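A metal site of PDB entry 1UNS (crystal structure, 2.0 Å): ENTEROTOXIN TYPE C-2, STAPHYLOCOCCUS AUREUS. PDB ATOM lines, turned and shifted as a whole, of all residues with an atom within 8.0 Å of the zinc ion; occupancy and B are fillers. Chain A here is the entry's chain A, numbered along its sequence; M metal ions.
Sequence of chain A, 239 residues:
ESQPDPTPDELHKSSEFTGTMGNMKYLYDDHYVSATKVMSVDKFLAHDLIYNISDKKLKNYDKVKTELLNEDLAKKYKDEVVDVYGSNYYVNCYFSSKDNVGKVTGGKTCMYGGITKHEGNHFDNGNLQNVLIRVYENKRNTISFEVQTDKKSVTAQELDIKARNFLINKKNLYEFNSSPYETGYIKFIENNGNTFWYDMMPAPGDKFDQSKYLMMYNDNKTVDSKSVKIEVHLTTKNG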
ATOM      1  N   ALA A  35     -15.301 -10.956  33.902  1.00  0.00           N
ATOM      2  CA  ALA A  35     -16.232 -11.288  32.832  1.00  0.00           C
ATOM      3  C   ALA A  35     -16.199 -10.168  31.799  1.00  0.00           C
ATOM      4  O   ALA A  35     -15.957  -9.012  32.122  1.00  0.00           O
ATOM      5  CB  ALA A  35     -17.642 -11.438  33.390  1.00  0.00           C
ATOM      6  N   THR A  36     -16.446 -10.533  30.548  1.00  0.00           N
ATOM      7  CA  THR A  36     -16.437  -9.560  29.464  1.00  0.00           C
ATOM      8  C   THR A  36     -17.750  -9.537  28.709  1.00  0.00           C
ATOM      9  O   THR A  36     -18.317 -10.588  28.387  1.00  0.00           O
ATOM     10  CB  THR A  36     -15.307  -9.855  28.453  1.00  0.00           C
ATOM     11  OG1 THR A  36     -14.039  -9.830  29.132  1.00  0.00           O
ATOM     12  CG2 THR A  36     -15.291  -8.805  27.351  1.00  0.00           C
ATOM     13  N   LYS A  37     -18.245  -8.336  28.442  1.00  0.00           N
ATOM     14  CA  LYS A  37     -19.470  -8.123  27.680  1.00  0.00           C
ATOM     15  C   LYS A  37     -20.662  -8.966  28.145  1.00  0.00           C
ATOM     16  O   LYS A  37     -21.249  -9.708  27.346  1.00  0.00           O
ATOM     17  CB  LYS A  37     -19.192  -8.372  26.201  1.00  0.00           C
ATOM     18  CG  LYS A  37     -18.233  -7.358  25.595  1.00  0.00           C
ATOM     19  CD  LYS A  37     -17.777  -7.746  24.198  1.00  0.00           C
ATOM     20  CE  LYS A  37     -18.944  -7.766  23.225  1.00  0.00           C
ATOM     21  NZ  LYS A  37     -18.502  -8.237  21.883  1.00  0.00           N
ATOM     22  N   VAL A  38     -21.016  -8.831  29.419  1.00  0.00           N
ATOM     23  CA  VAL A  38     -22.136  -9.556  29.981  1.00  0.00           C
ATOM     24  C   VAL A  38     -23.258  -8.586  30.343  1.00  0.00           C
ATOM     25  O   VAL A  38     -23.054  -7.367  30.400  1.00  0.00           O
ATOM     26  CB  VAL A  38     -21.717 -10.357  31.247  1.00  0.00           C
ATOM     27  CG1 VAL A  38     -20.772 -11.479  30.847  1.00  0.00           C
ATOM     28  CG2 VAL A  38     -21.046  -9.431  32.257  1.00  0.00           C
ATOM     29  N   VAL A  81     -24.383  -3.635  28.373  1.00  0.00           N
ATOM     30  CA  VAL A  81     -23.387  -4.672  28.192  1.00  0.00           C
ATOM     31  C   VAL A  81     -22.175  -4.164  28.978  1.00  0.00           C
ATOM     32  O   VAL A  81     -21.627  -3.113  28.667  1.00  0.00           O
ATOM     33  CB  VAL A  81     -23.020  -4.834  26.702  1.00  0.00           C
ATOM     34  CG1 VAL A  81     -21.884  -5.854  26.529  1.00  0.00           C
ATOM     35  CG2 VAL A  81     -24.242  -5.286  25.918  1.00  0.00           C
ATOM     36  N   VAL A  82     -21.780  -4.910  30.000  1.00  0.00           N
ATOM     37  CA  VAL A  82     -20.671  -4.494  30.855  1.00  0.00           C
ATOM     38  C   VAL A  82     -19.550  -5.513  31.049  1.00  0.00           C
ATOM     39  O   VAL A  82     -19.660  -6.686  30.683  1.00  0.00           O
ATOM     40  CB  VAL A  82     -21.179  -4.117  32.262  1.00  0.00           C
ATOM     41  CG1 VAL A  82     -22.250  -3.060  32.165  1.00  0.00           C
ATOM     42  CG2 VAL A  82     -21.725  -5.363  32.956  1.00  0.00           C
ATOM     43  N   ASP A  83     -18.460  -5.021  31.641  1.00  0.00           N
ATOM     44  CA  ASP A  83     -17.307  -5.838  31.971  1.00  0.00           C
ATOM     45  C   ASP A  83     -17.307  -5.908  33.491  1.00  0.00           C
ATOM     46  O   ASP A  83     -17.703  -4.958  34.154  1.00  0.00           O
ATOM     47  CB  ASP A  83     -16.017  -5.182  31.488  1.00  0.00           C
ATOM     48  CG  ASP A  83     -15.882  -5.199  29.984  1.00  0.00           C
ATOM     49  OD1 ASP A  83     -15.133  -4.355  29.456  1.00  0.00           O
ATOM     50  OD2 ASP A  83     -16.495  -6.071  29.333  1.00  0.00           O
ATOM     51  N   VAL A  84     -16.860  -7.026  34.044  1.00  0.00           N
ATOM     52  CA  VAL A  84     -16.847  -7.196  35.492  1.00  0.00           C
ATOM     53  C   VAL A  84     -15.490  -7.620  36.015  1.00  0.00           C
ATOM     54  O   VAL A  84     -14.824  -8.468  35.419  1.00  0.00           O
ATOM     55  CB  VAL A  84     -17.877  -8.270  35.936  1.00  0.00           C
ATOM     56  CG1 VAL A  84     -17.876  -8.405  37.448  1.00  0.00           C
ATOM     57  CG2 VAL A  84     -19.252  -7.903  35.437  1.00  0.00           C
ATOM     58  N   THR A 116     -18.082  -1.921  34.877  1.00  0.00           N
ATOM     59  CA  THR A 116     -17.747  -0.841  33.959  1.00  0.00           C
ATOM     60  C   THR A 116     -18.356  -1.148  32.593  1.00  0.00           C
ATOM     61  O   THR A 116     -18.393  -2.301  32.156  1.00  0.00           O
ATOM     62  CB  THR A 116     -16.215  -0.648  33.779  1.00  0.00           C
ATOM     63  OG1 THR A 116     -15.602  -1.887  33.421  1.00  0.00           O
ATOM     64  CG2 THR A 116     -15.599  -0.104  35.067  1.00  0.00           C
ATOM     65  N   LYS A 117     -18.853  -0.108  31.936  1.00  0.00           N
ATOM     66  CA  LYS A 117     -19.452  -0.229  30.616  1.00  0.00           C
ATOM     67  C   LYS A 117     -18.353  -0.776  29.692  1.00  0.00           C
ATOM     68  O   LYS A 117     -17.197  -0.370  29.803  1.00  0.00           O
ATOM     69  CB  LYS A 117     -19.897   1.161  30.166  1.00  0.00           C
ATOM     70  CG  LYS A 117     -20.727   1.241  28.898  1.00  0.00           C
ATOM     71  CD  LYS A 117     -21.135   2.698  28.633  1.00  0.00           C
ATOM     72  CE  LYS A 117     -22.007   2.845  27.399  1.00  0.00           C
ATOM     73  NZ  LYS A 117     -22.320   4.275  27.111  1.00  0.00           N
ATOM     74  N   HIS A 118     -18.692  -1.693  28.798  1.00  0.00           N
ATOM     75  CA  HIS A 118     -17.691  -2.221  27.879  1.00  0.00           C
ATOM     76  C   HIS A 118     -17.435  -1.255  26.713  1.00  0.00           C
ATOM     77  O   HIS A 118     -16.285  -1.003  26.334  1.00  0.00           O
ATOM     78  CB  HIS A 118     -18.136  -3.578  27.323  1.00  0.00           C
ATOM     79  CG  HIS A 118     -17.404  -3.998  26.087  1.00  0.00           C
ATOM     80  ND1 HIS A 118     -16.121  -4.487  26.117  1.00  0.00           N
ATOM     81  CD2 HIS A 118     -17.766  -3.955  24.784  1.00  0.00           C
ATOM     82  CE1 HIS A 118     -15.716  -4.740  24.881  1.00  0.00           C
ATOM     83  NE2 HIS A 118     -16.694  -4.430  24.051  1.00  0.00           N
ATOM     84  N   GLU A 119     -18.531  -0.711  26.166  1.00  0.00           N
ATOM     85  CA  GLU A 119     -18.452   0.226  25.044  1.00  0.00           C
ATOM     86  C   GLU A 119     -17.639   1.477  25.303  1.00  0.00           C
ATOM     87  O   GLU A 119     -17.875   2.168  26.300  1.00  0.00           O
ATOM     88  CB  GLU A 119     -19.853   0.661  24.630  1.00  0.00           C
ATOM     89  CG  GLU A 119     -20.727  -0.429  24.104  1.00  0.00           C
ATOM     90  CD  GLU A 119     -22.156   0.041  23.981  1.00  0.00           C
ATOM     91  OE1 GLU A 119     -22.756   0.378  25.028  1.00  0.00           O
ATOM     92  OE2 GLU A 119     -22.669   0.083  22.838  1.00  0.00           O
ATOM     93  N   GLY A 120     -16.717   1.771  24.399  1.00  0.00           N
ATOM     94  CA  GLY A 120     -15.882   2.959  24.507  1.00  0.00           C
ATOM     95  C   GLY A 120     -15.000   3.034  25.742  1.00  0.00           C
ATOM     96  O   GLY A 120     -14.527   4.114  26.097  1.00  0.00           O
ATOM     97  N   ASN A 121     -14.753   1.901  26.401  1.00  0.00           N
ATOM     98  CA  ASN A 121     -13.919   1.930  27.596  1.00  0.00           C
ATOM     99  C   ASN A 121     -12.545   1.264  27.433  1.00  0.00           C
ATOM    100  O   ASN A 121     -11.855   0.992  28.425  1.00  0.00           O
ATOM    101  CB  ASN A 121     -14.656   1.264  28.775  1.00  0.00           C
ATOM    102  CG  ASN A 121     -14.058   1.630  30.111  1.00  0.00           C
ATOM    103  OD1 ASN A 121     -14.028   0.818  31.033  1.00  0.00           O
ATOM    104  ND2 ASN A 121     -13.575   2.854  30.228  1.00  0.00           N
ATOM    105  N   HIS A 122     -12.147   1.015  26.186  1.00  0.00           N
ATOM    106  CA  HIS A 122     -10.842   0.393  25.908  1.00  0.00           C
ATOM    107  C   HIS A 122      -9.972   1.259  25.003  1.00  0.00           C
ATOM    108  O   HIS A 122     -10.472   2.092  24.251  1.00  0.00           O
ATOM    109  CB  HIS A 122     -11.045  -0.998  25.281  1.00  0.00           C
ATOM    110  CG  HIS A 122     -11.811  -1.946  26.161  1.00  0.00           C
ATOM    111  ND1 HIS A 122     -11.339  -2.361  27.394  1.00  0.00           N
ATOM    112  CD2 HIS A 122     -13.024  -2.519  26.012  1.00  0.00           C
ATOM    113  CE1 HIS A 122     -12.233  -3.151  27.952  1.00  0.00           C
ATOM    114  NE2 HIS A 122     -13.273  -3.263  27.137  1.00  0.00           N
ATOM    115  N   ASP A 150      -6.818  -2.869  30.879  1.00  0.00           N
ATOM    116  CA  ASP A 150      -7.191  -2.574  29.505  1.00  0.00           C
ATOM    117  C   ASP A 150      -8.343  -1.574  29.462  1.00  0.00           C
ATOM    118  O   ASP A 150      -8.851  -1.239  28.402  1.00  0.00           O
ATOM    119  CB  ASP A 150      -7.609  -3.863  28.802  1.00  0.00           C
ATOM    120  CG  ASP A 150      -8.806  -4.529  29.460  1.00  0.00           C
ATOM    121  OD1 ASP A 150      -9.424  -5.389  28.816  1.00  0.00           O
ATOM    122  OD2 ASP A 150      -9.121  -4.204  30.626  1.00  0.00           O
ATOM    123  N   LYS A 151      -8.756  -1.090  30.634  1.00  0.00           N
ATOM    124  CA  LYS A 151      -9.862  -0.147  30.724  1.00  0.00           C
ATOM    125  C   LYS A 151      -9.428   1.317  30.919  1.00  0.00           C
ATOM    126  O   LYS A 151      -8.470   1.585  31.643  1.00  0.00           O
ATOM    127  CB  LYS A 151     -10.774  -0.536  31.898  1.00  0.00           C
ATOM    128  CG  LYS A 151     -11.252  -1.976  31.861  1.00  0.00           C
ATOM    129  CD  LYS A 151     -12.107  -2.307  33.092  1.00  0.00           C
ATOM    130  CE  LYS A 151     -12.614  -3.744  33.046  1.00  0.00           C
ATOM    131  NZ  LYS A 151     -11.538  -4.743  33.292  1.00  0.00           N
HETATM  132 ZN    ZN M   1     -14.671  -4.632  27.620  1.00  0.00          ZN
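ND1 of His 122 is in hydrogen-bond range of O of Asp 150 (2.9 Å). OD2 of Asp 83 sits at hydrogen-bond distance from N of Lys 37 (3.0 Å). The backbone carbonyl oxygen (O) of Thr 116 sits at hydrogen-bond distance from the backbone NH (N) of Asp 83 (2.8 Å). The backbone NH (N) of His 118 lies within hydrogen-bond range of the backbone carbonyl oxygen (O) of Val 81, 3.3 Å away.
The zinc ion is bound by OD1 of Asp 83 (1.9 Å). The zinc ion is bound by NE2 of His 122 (2.0 Å). The zinc ion is bound by ND1 of His 118 (2.1 Å).
Three residues have an atom within 4 Å of the zinc ion: Asp 83, His 118 and His 122. Along chain A the residues within 4 Å of the zinc ion span positions 83 to 122. The nearest printed residue that does not touch the zinc ion is Thr 36 (4.2 Å).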
